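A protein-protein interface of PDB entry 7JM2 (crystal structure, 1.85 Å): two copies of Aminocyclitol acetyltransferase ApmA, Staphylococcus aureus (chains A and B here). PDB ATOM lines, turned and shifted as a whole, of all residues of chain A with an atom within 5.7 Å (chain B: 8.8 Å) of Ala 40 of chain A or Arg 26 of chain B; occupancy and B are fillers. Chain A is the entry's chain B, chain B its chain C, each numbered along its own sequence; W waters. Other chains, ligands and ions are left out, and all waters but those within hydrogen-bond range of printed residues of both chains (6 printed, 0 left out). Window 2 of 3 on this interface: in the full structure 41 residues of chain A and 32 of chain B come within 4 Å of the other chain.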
ATOM      1  N   ALA A  19     -17.832 -39.347  25.140  1.00  0.00           N
ATOM      2  CA  ALA A  19     -18.428 -38.061  25.492  1.00  0.00           C
ATOM      3  C   ALA A  19     -17.532 -36.977  24.919  1.00  0.00           C
ATOM      4  O   ALA A  19     -16.389 -36.814  25.359  1.00  0.00           O
ATOM      5  CB  ALA A  19     -18.568 -37.920  27.005  1.00  0.00           C
ATOM      6  N   VAL A  20     -18.030 -36.232  23.944  1.00  0.00           N
ATOM      7  CA  VAL A  20     -17.196 -35.249  23.259  1.00  0.00           C
ATOM      8  C   VAL A  20     -17.225 -33.933  24.028  1.00  0.00           C
ATOM      9  O   VAL A  20     -18.266 -33.268  24.109  1.00  0.00           O
ATOM     10  CB  VAL A  20     -17.644 -35.043  21.807  1.00  0.00           C
ATOM     11  CG1 VAL A  20     -16.813 -33.924  21.178  1.00  0.00           C
ATOM     12  CG2 VAL A  20     -17.504 -36.335  21.038  1.00  0.00           C
ATOM     13  N   TRP A  21     -16.063 -33.545  24.548  1.00  0.00           N
ATOM     14  CA  TRP A  21     -15.872 -32.307  25.299  1.00  0.00           C
ATOM     15  C   TRP A  21     -15.316 -31.279  24.319  1.00  0.00           C
ATOM     16  O   TRP A  21     -14.112 -31.201  24.090  1.00  0.00           O
ATOM     17  CB  TRP A  21     -14.931 -32.536  26.477  1.00  0.00           C
ATOM     18  CG  TRP A  21     -15.089 -31.567  27.625  1.00  0.00           C
ATOM     19  CD1 TRP A  21     -14.549 -30.318  27.727  1.00  0.00           C
ATOM     20  CD2 TRP A  21     -15.823 -31.788  28.833  1.00  0.00           C
ATOM     21  NE1 TRP A  21     -14.909 -29.741  28.927  1.00  0.00           N
ATOM     22  CE2 TRP A  21     -15.692 -30.625  29.621  1.00  0.00           C
ATOM     23  CE3 TRP A  21     -16.584 -32.853  29.325  1.00  0.00           C
ATOM     24  CZ2 TRP A  21     -16.289 -30.502  30.878  1.00  0.00           C
ATOM     25  CZ3 TRP A  21     -17.182 -32.725  30.577  1.00  0.00           C
ATOM     26  CH2 TRP A  21     -17.028 -31.557  31.335  1.00  0.00           C
ATOM     27  N   GLY A  22     -16.208 -30.496  23.732  1.00  0.00           N
ATOM     28  CA  GLY A  22     -15.837 -29.454  22.797  1.00  0.00           C
ATOM     29  C   GLY A  22     -16.672 -29.530  21.536  1.00  0.00           C
ATOM     30  O   GLY A  22     -17.478 -30.437  21.338  1.00  0.00           O
ATOM     31  N   VAL A  23     -16.468 -28.537  20.679  1.00  0.00           N
ATOM     32  CA  VAL A  23     -17.191 -28.493  19.411  1.00  0.00           C
ATOM     33  C   VAL A  23     -16.572 -29.516  18.471  1.00  0.00           C
ATOM     34  O   VAL A  23     -15.368 -29.449  18.193  1.00  0.00           O
ATOM     35  CB  VAL A  23     -17.177 -27.089  18.788  1.00  0.00           C
ATOM     36  CG1 VAL A  23     -18.093 -27.061  17.575  1.00  0.00           C
ATOM     37  CG2 VAL A  23     -17.609 -26.047  19.814  1.00  0.00           C
ATOM     38  N   HIS A  38     -21.701 -38.825  21.941  1.00  0.00           N
ATOM     39  CA  HIS A  38     -22.658 -37.768  22.249  1.00  0.00           C
ATOM     40  C   HIS A  38     -21.901 -36.562  22.797  1.00  0.00           C
ATOM     41  O   HIS A  38     -20.754 -36.672  23.234  1.00  0.00           O
ATOM     42  CB  HIS A  38     -23.703 -38.242  23.263  1.00  0.00           C
ATOM     43  CG  HIS A  38     -23.113 -38.635  24.582  1.00  0.00           C
ATOM     44  ND1 HIS A  38     -22.965 -37.747  25.627  1.00  0.00           N
ATOM     45  CD2 HIS A  38     -22.613 -39.816  25.018  1.00  0.00           C
ATOM     46  CE1 HIS A  38     -22.400 -38.365  26.650  1.00  0.00           C
ATOM     47  NE2 HIS A  38     -22.177 -39.620  26.308  1.00  0.00           N
ATOM     48  N   THR A  39     -22.564 -35.405  22.776  1.00  0.00           N
ATOM     49  CA  THR A  39     -22.008 -34.201  23.383  1.00  0.00           C
ATOM     50  C   THR A  39     -21.929 -34.371  24.898  1.00  0.00           C
ATOM     51  O   THR A  39     -22.928 -34.695  25.549  1.00  0.00           O
ATOM     52  CB  THR A  39     -22.874 -32.991  23.030  1.00  0.00           C
ATOM     53  OG1 THR A  39     -22.972 -32.875  21.608  1.00  0.00           O
ATOM     54  CG2 THR A  39     -22.271 -31.712  23.586  1.00  0.00           C
ATOM     55  N   ALA A  40     -20.744 -34.151  25.462  1.00  0.00           N
ATOM     56  CA  ALA A  40     -20.544 -34.387  26.884  1.00  0.00           C
ATOM     57  C   ALA A  40     -21.301 -33.367  27.724  1.00  0.00           C
ATOM     58  O   ALA A  40     -21.365 -32.180  27.388  1.00  0.00           O
ATOM     59  CB  ALA A  40     -19.058 -34.335  27.231  1.00  0.00           C
ATOM     60  N   ASP A  41     -21.887 -33.841  28.822  1.00  0.00           N
ATOM     61  CA  ASP A  41     -22.485 -32.948  29.806  1.00  0.00           C
ATOM     62  C   ASP A  41     -22.099 -33.428  31.196  1.00  0.00           C
ATOM     63  O   ASP A  41     -21.105 -32.973  31.768  1.00  0.00           O
ATOM     64  CB  ASP A  41     -24.006 -32.892  29.634  1.00  0.00           C
ATOM     65  CG  ASP A  41     -24.645 -31.738  30.404  1.00  0.00           C
ATOM     66  OD1 ASP A  41     -24.302 -31.533  31.592  1.00  0.00           O
ATOM     67  OD2 ASP A  41     -25.496 -31.033  29.818  1.00  0.00           O
ATOM     68  N   ARG A  42     -22.877 -34.343  31.753  1.00  0.00           N
ATOM     69  CA  ARG A  42     -22.464 -35.058  32.950  1.00  0.00           C
ATOM     70  C   ARG A  42     -21.743 -36.318  32.500  1.00  0.00           C
ATOM     71  O   ARG A  42     -22.268 -37.077  31.681  1.00  0.00           O
ATOM     72  CB  ARG A  42     -23.668 -35.394  33.823  1.00  0.00           C
ATOM     73  CG  ARG A  42     -24.393 -34.167  34.322  1.00  0.00           C
ATOM     74  CD  ARG A  42     -23.485 -33.300  35.177  1.00  0.00           C
ATOM     75  NE  ARG A  42     -22.982 -34.027  36.339  1.00  0.00           N
ATOM     76  CZ  ARG A  42     -22.361 -33.451  37.362  1.00  0.00           C
ATOM     77  NH1 ARG A  42     -22.178 -32.139  37.364  1.00  0.00           N
ATOM     78  NH2 ARG A  42     -21.929 -34.182  38.383  1.00  0.00           N
ATOM     79  N   VAL A  43     -20.531 -36.525  33.003  1.00  0.00           N
ATOM     80  CA  VAL A  43     -19.697 -37.625  32.545  1.00  0.00           C
ATOM     81  C   VAL A  43     -19.299 -38.480  33.737  1.00  0.00           C
ATOM     82  O   VAL A  43     -19.074 -37.970  34.840  1.00  0.00           O
ATOM     83  CB  VAL A  43     -18.454 -37.132  31.770  1.00  0.00           C
ATOM     84  CG1 VAL A  43     -18.872 -36.582  30.427  1.00  0.00           C
ATOM     85  CG2 VAL A  43     -17.689 -36.084  32.566  1.00  0.00           C
ATOM     86  N   VAL A  50     -14.007 -39.722  27.684  1.00  0.00           N
ATOM     87  CA  VAL A  50     -14.081 -38.311  27.300  1.00  0.00           C
ATOM     88  C   VAL A  50     -13.041 -38.003  26.227  1.00  0.00           C
ATOM     89  O   VAL A  50     -11.844 -38.277  26.394  1.00  0.00           O
ATOM     90  CB  VAL A  50     -13.906 -37.389  28.525  1.00  0.00           C
ATOM     91  CG1 VAL A  50     -13.748 -35.948  28.070  1.00  0.00           C
ATOM     92  CG2 VAL A  50     -15.108 -37.489  29.435  1.00  0.00           C
ATOM     93  N   ASP A  57      -9.897 -27.327  24.984  1.00  0.00           N
ATOM     94  CA  ASP A  57     -10.974 -28.128  25.551  1.00  0.00           C
ATOM     95  C   ASP A  57     -10.471 -29.024  26.674  1.00  0.00           C
ATOM     96  O   ASP A  57     -11.174 -29.227  27.669  1.00  0.00           O
ATOM     97  CB  ASP A  57     -11.626 -28.988  24.474  1.00  0.00           C
ATOM     98  CG  ASP A  57     -12.368 -28.173  23.440  1.00  0.00           C
ATOM     99  OD1 ASP A  57     -12.926 -27.113  23.794  1.00  0.00           O
ATOM    100  OD2 ASP A  57     -12.383 -28.609  22.269  1.00  0.00           O
ATOM    101  N   ASP A  60     -10.093 -27.246  29.878  1.00  0.00           N
ATOM    102  CA  ASP A  60     -11.377 -27.014  30.527  1.00  0.00           C
ATOM    103  C   ASP A  60     -11.874 -28.273  31.225  1.00  0.00           C
ATOM    104  O   ASP A  60     -12.375 -28.203  32.353  1.00  0.00           O
ATOM    105  CB  ASP A  60     -12.401 -26.526  29.503  1.00  0.00           C
ATOM    106  CG  ASP A  60     -13.742 -26.215  30.137  1.00  0.00           C
ATOM    107  OD1 ASP A  60     -14.669 -27.052  30.024  1.00  0.00           O
ATOM    108  OD2 ASP A  60     -13.849 -25.143  30.775  1.00  0.00           O
ATOM    109  N   VAL B  23     -17.812 -18.249  17.096  1.00  0.00           N
ATOM    110  CA  VAL B  23     -18.294 -19.523  17.627  1.00  0.00           C
ATOM    111  C   VAL B  23     -17.746 -19.677  19.040  1.00  0.00           C
ATOM    112  O   VAL B  23     -16.529 -19.583  19.245  1.00  0.00           O
ATOM    113  CB  VAL B  23     -17.891 -20.706  16.733  1.00  0.00           C
ATOM    114  CG1 VAL B  23     -18.189 -22.021  17.439  1.00  0.00           C
ATOM    115  CG2 VAL B  23     -18.637 -20.649  15.407  1.00  0.00           C
ATOM    116  N   PRO B  24     -18.592 -19.884  20.040  1.00  0.00           N
ATOM    117  CA  PRO B  24     -18.087 -20.040  21.406  1.00  0.00           C
ATOM    118  C   PRO B  24     -17.460 -21.410  21.618  1.00  0.00           C
ATOM    119  O   PRO B  24     -17.734 -22.380  20.906  1.00  0.00           O
ATOM    120  CB  PRO B  24     -19.339 -19.857  22.269  1.00  0.00           C
ATOM    121  CG  PRO B  24     -20.456 -20.311  21.384  1.00  0.00           C
ATOM    122  CD  PRO B  24     -20.064 -19.928  19.979  1.00  0.00           C
ATOM    123  N   THR B  25     -16.584 -21.466  22.617  1.00  0.00           N
ATOM    124  CA  THR B  25     -15.853 -22.662  23.002  1.00  0.00           C
ATOM    125  C   THR B  25     -16.234 -23.038  24.428  1.00  0.00           C
ATOM    126  O   THR B  25     -16.861 -22.258  25.147  1.00  0.00           O
ATOM    127  CB  THR B  25     -14.337 -22.432  22.914  1.00  0.00           C
ATOM    128  OG1 THR B  25     -13.950 -21.457  23.904  1.00  0.00           O
ATOM    129  CG2 THR B  25     -13.950 -21.938  21.525  1.00  0.00           C
ATOM    130  N   ARG B  26     -15.822 -24.242  24.840  1.00  0.00           N
ATOM    131  CA  ARG B  26     -16.118 -24.693  26.198  1.00  0.00           C
ATOM    132  C   ARG B  26     -15.519 -23.745  27.225  1.00  0.00           C
ATOM    133  O   ARG B  26     -16.182 -23.363  28.199  1.00  0.00           O
ATOM    134  CB  ARG B  26     -15.581 -26.107  26.414  1.00  0.00           C
ATOM    135  CG  ARG B  26     -16.462 -27.189  25.835  1.00  0.00           C
ATOM    136  CD  ARG B  26     -17.305 -27.815  26.903  1.00  0.00           C
ATOM    137  NE  ARG B  26     -18.259 -28.754  26.339  1.00  0.00           N
ATOM    138  CZ  ARG B  26     -18.940 -29.639  27.058  1.00  0.00           C
ATOM    139  NH1 ARG B  26     -18.763 -29.696  28.366  1.00  0.00           N
ATOM    140  NH2 ARG B  26     -19.793 -30.461  26.469  1.00  0.00           N
ATOM    141  N   ARG B  27     -14.266 -23.344  27.019  1.00  0.00           N
ATOM    142  CA  ARG B  27     -13.592 -22.515  28.013  1.00  0.00           C
ATOM    143  C   ARG B  27     -14.153 -21.100  28.056  1.00  0.00           C
ATOM    144  O   ARG B  27     -14.158 -20.468  29.118  1.00  0.00           O
ATOM    145  CB  ARG B  27     -12.091 -22.484  27.738  1.00  0.00           C
ATOM    146  CG  ARG B  27     -11.309 -22.225  28.991  1.00  0.00           C
ATOM    147  CD  ARG B  27      -9.842 -22.474  28.822  1.00  0.00           C
ATOM    148  NE  ARG B  27      -9.087 -21.348  29.347  1.00  0.00           N
ATOM    149  CZ  ARG B  27      -8.582 -20.385  28.588  1.00  0.00           C
ATOM    150  NH1 ARG B  27      -8.751 -20.426  27.275  1.00  0.00           N
ATOM    151  NH2 ARG B  27      -7.911 -19.383  29.143  1.00  0.00           N
ATOM    152  N   LEU B  28     -14.642 -20.594  26.926  1.00  0.00           N
ATOM    153  CA  LEU B  28     -15.283 -19.286  26.941  1.00  0.00           C
ATOM    154  C   LEU B  28     -16.582 -19.323  27.741  1.00  0.00           C
ATOM    155  O   LEU B  28     -16.859 -18.416  28.534  1.00  0.00           O
ATOM    156  CB  LEU B  28     -15.545 -18.805  25.513  1.00  0.00           C
ATOM    157  CG  LEU B  28     -16.334 -17.493  25.463  1.00  0.00           C
ATOM    158  CD1 LEU B  28     -15.580 -16.392  26.198  1.00  0.00           C
ATOM    159  CD2 LEU B  28     -16.633 -17.078  24.050  1.00  0.00           C
ATOM    160  N   LEU B  29     -17.391 -20.364  27.550  1.00  0.00           N
ATOM    161  CA  LEU B  29     -18.657 -20.431  28.268  1.00  0.00           C
ATOM    162  C   LEU B  29     -18.430 -20.605  29.765  1.00  0.00           C
ATOM    163  O   LEU B  29     -19.223 -20.108  30.574  1.00  0.00           O
ATOM    164  CB  LEU B  29     -19.523 -21.557  27.698  1.00  0.00           C
ATOM    165  CG  LEU B  29     -19.910 -21.353  26.229  1.00  0.00           C
ATOM    166  CD1 LEU B  29     -20.547 -22.593  25.637  1.00  0.00           C
ATOM    167  CD2 LEU B  29     -20.831 -20.151  26.063  1.00  0.00           C
ATOM    168  N   ARG B  30     -17.343 -21.279  30.153  1.00  0.00           N
ATOM    169  CA  ARG B  30     -16.982 -21.334  31.567  1.00  0.00           C
ATOM    170  C   ARG B  30     -16.626 -19.951  32.097  1.00  0.00           C
ATOM    171  O   ARG B  30     -17.012 -19.592  33.217  1.00  0.00           O
ATOM    172  CB  ARG B  30     -15.819 -22.304  31.786  1.00  0.00           C
ATOM    173  CG  ARG B  30     -15.277 -22.341  33.213  1.00  0.00           C
ATOM    174  CD  ARG B  30     -15.810 -23.554  33.956  1.00  0.00           C
ATOM    175  NE  ARG B  30     -15.455 -24.808  33.296  1.00  0.00           N
ATOM    176  CZ  ARG B  30     -15.851 -26.003  33.714  1.00  0.00           C
ATOM    177  NH1 ARG B  30     -16.617 -26.111  34.793  1.00  0.00           N
ATOM    178  NH2 ARG B  30     -15.483 -27.091  33.054  1.00  0.00           N
ATOM    179  N   ALA B  31     -15.905 -19.153  31.304  1.00  0.00           N
ATOM    180  CA  ALA B  31     -15.492 -17.834  31.779  1.00  0.00           C
ATOM    181  C   ALA B  31     -16.665 -16.865  31.853  1.00  0.00           C
ATOM    182  O   ALA B  31     -16.631 -15.916  32.643  1.00  0.00           O
ATOM    183  CB  ALA B  31     -14.396 -17.269  30.874  1.00  0.00           C
ATOM    184  N   LEU B  32     -17.704 -17.085  31.047  1.00  0.00           N
ATOM    185  CA  LEU B  32     -18.820 -16.158  30.927  1.00  0.00           C
ATOM    186  C   LEU B  32     -19.974 -16.466  31.871  1.00  0.00           C
ATOM    187  O   LEU B  32     -20.935 -15.691  31.907  1.00  0.00           O
ATOM    188  CB  LEU B  32     -19.347 -16.150  29.485  1.00  0.00           C
ATOM    189  CG  LEU B  32     -18.493 -15.442  28.429  1.00  0.00           C
ATOM    190  CD1 LEU B  32     -19.226 -15.431  27.083  1.00  0.00           C
ATOM    191  CD2 LEU B  32     -18.160 -14.034  28.865  1.00  0.00           C
ATOM    192  N   LYS B  33     -19.918 -17.569  32.619  1.00  0.00           N
ATOM    193  CA  LYS B  33     -21.069 -17.960  33.431  1.00  0.00           C
ATOM    194  C   LYS B  33     -21.521 -16.883  34.414  1.00  0.00           C
ATOM    195  O   LYS B  33     -22.744 -16.700  34.555  1.00  0.00           O
ATOM    196  CB  LYS B  33     -20.773 -19.274  34.169  1.00  0.00           C
ATOM    197  CG  LYS B  33     -22.018 -19.953  34.748  1.00  0.00           C
ATOM    198  CD  LYS B  33     -21.961 -20.063  36.273  1.00  0.00           C
ATOM    199  CE  LYS B  33     -22.372 -18.769  36.959  1.00  0.00           C
ATOM    200  NZ  LYS B  33     -22.703 -18.942  38.401  1.00  0.00           N
ATOM    201  N   VAL B  53     -14.140 -14.211  20.011  1.00  0.00           N
ATOM    202  CA  VAL B  53     -13.637 -15.489  20.508  1.00  0.00           C
ATOM    203  C   VAL B  53     -12.179 -15.686  20.098  1.00  0.00           C
ATOM    204  O   VAL B  53     -11.300 -15.887  20.943  1.00  0.00           O
ATOM    205  CB  VAL B  53     -14.520 -16.649  20.018  1.00  0.00           C
ATOM    206  CG1 VAL B  53     -14.012 -17.966  20.581  1.00  0.00           C
ATOM    207  CG2 VAL B  53     -15.950 -16.415  20.427  1.00  0.00           C
ATOM    208  N   PHE B  79     -11.073 -13.257  23.456  1.00  0.00           N
ATOM    209  CA  PHE B  79     -10.980 -14.245  24.525  1.00  0.00           C
ATOM    210  C   PHE B  79      -9.682 -15.041  24.440  1.00  0.00           C
ATOM    211  O   PHE B  79      -8.994 -15.230  25.450  1.00  0.00           O
ATOM    212  CB  PHE B  79     -12.165 -15.198  24.503  1.00  0.00           C
ATOM    213  CG  PHE B  79     -12.050 -16.286  25.526  1.00  0.00           C
ATOM    214  CD1 PHE B  79     -12.006 -15.972  26.877  1.00  0.00           C
ATOM    215  CD2 PHE B  79     -11.946 -17.612  25.149  1.00  0.00           C
ATOM    216  CE1 PHE B  79     -11.882 -16.963  27.828  1.00  0.00           C
ATOM    217  CE2 PHE B  79     -11.820 -18.607  26.102  1.00  0.00           C
ATOM    218  CZ  PHE B  79     -11.786 -18.283  27.436  1.00  0.00           C
HETATM  219  O   HOH W   1     -17.098 -26.917  30.311  1.00  0.00           O
HETATM  220  O   HOH W   2     -15.020 -25.937  22.745  1.00  0.00           O
HETATM  221  O   HOH W   3     -22.732 -29.658  27.361  1.00  0.00           O
HETATM  222  O   HOH W   4     -12.598 -24.766  25.141  1.00  0.00           O
HETATM  223  O   HOH W   5     -20.073 -30.738  30.403  1.00  0.00           O
HETATM  224  O   HOH W   6     -18.869 -30.445  24.045  1.00  0.00           O
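OD2 of Asp 60 of chain A is in salt-bridge range of NE of Arg 30 of chain B (3.0 Å).
The guanidinium group of Arg 26 of chain B lies within hydrogen-bond range of the backbone carbonyl oxygen of Ala 40 of chain A, 2.5 Å away.
Printed residues of chain B within 4 Å of Val 20 of chain A: Arg 26.
Of the printed residues of chain B, Gly 22 of chain A touches Arg 26 (3.7 Å).
Of the printed residues of chain B, Asp 57 of chain A touches Arg 26.
Of the printed residues of chain B, Asp 60 of chain A touches Arg 26, Arg 27 and Arg 30.
Of the printed residues of chain A, Arg 26 of chain B touches Val 20 (3.97 Å), Trp 21 (3.4 Å), Gly 22 (3.7 Å), Ala 40 (2.5 Å), Asp 57 (3.9 Å) and Asp 60 (3.8 Å).
Of the printed residues of chain A, Arg 27 of chain B touches Asp 60 (3.8 Å).
The nearest printed residue of chain B that does not touch Ala 40 of chain A is Arg 30 of chain B (9.6 Å).
The indole nitrogen of Trp 21 of chain A is in hydrogen-bond range of the side-chain carboxylate of Asp 60 of chain A (2.9 Å).
N of Val 20 of chain A sits at hydrogen-bond distance from O of His 38 of chain A.
O of Val 20 of chain A sits at hydrogen-bond distance from N of Ala 40 of chain A.
Water W1 lies within hydrogen-bond range of the side-chain carboxylate of Asp 60 of chain A (2.4 Å) and the guanidinium group of Arg 30 of chain B (3.2 Å).
Water W6 lies within hydrogen-bond range of NH2 of Arg 26 of chain B (2.6 Å), N of Gly 22 of chain A (2.7 Å) and O of Val 20 of chain A (2.9 Å).
Water W2 bridges OD1 of Asp 57 of chain A (2.6 Å) and N of Arg 26 of chain B (2.8 Å).
Water W5 bridges NH1 of Arg 26 of chain B (2.6 Å) and O of Asp 41 of chain A (2.8 Å).
Water W4 lies within hydrogen-bond range of OD1 of Asp 57 of chain A (2.7 Å), N of Arg 27 of chain B (2.9 Å) and N of Arg 26 of chain B (3.3 Å).
Water W3 lies within hydrogen-bond range of O of Ala 40 of chain A and NH2 of Arg 26 of chain B.
NH2 of Arg 26 of chain B touches O of Val 20 of chain A, 3.97 Å away.
NH1 of Arg 26 of chain B touches CE2 of Trp 21 of chain A, 3.4 Å away.
Gly 22 of chain A touches Arg 26 of chain B.
Pro 24 of chain B touches Val 23 of chain A.
CB of Arg 26 of chain B touches OD1 of Asp 57 of chain A, 3.9 Å away.
Arg 26 of chain B touches Asp 60 of chain A (CB to OD1, 3.8 Å).
OD2 of Asp 60 of chain A touches CA of Arg 27 of chain B, at 3.8 Å.
Position printed for both chains: 23.
Of the 9 pairs that touch across the chains among the printed residues, none has its exchanged pair printed and touching as well.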
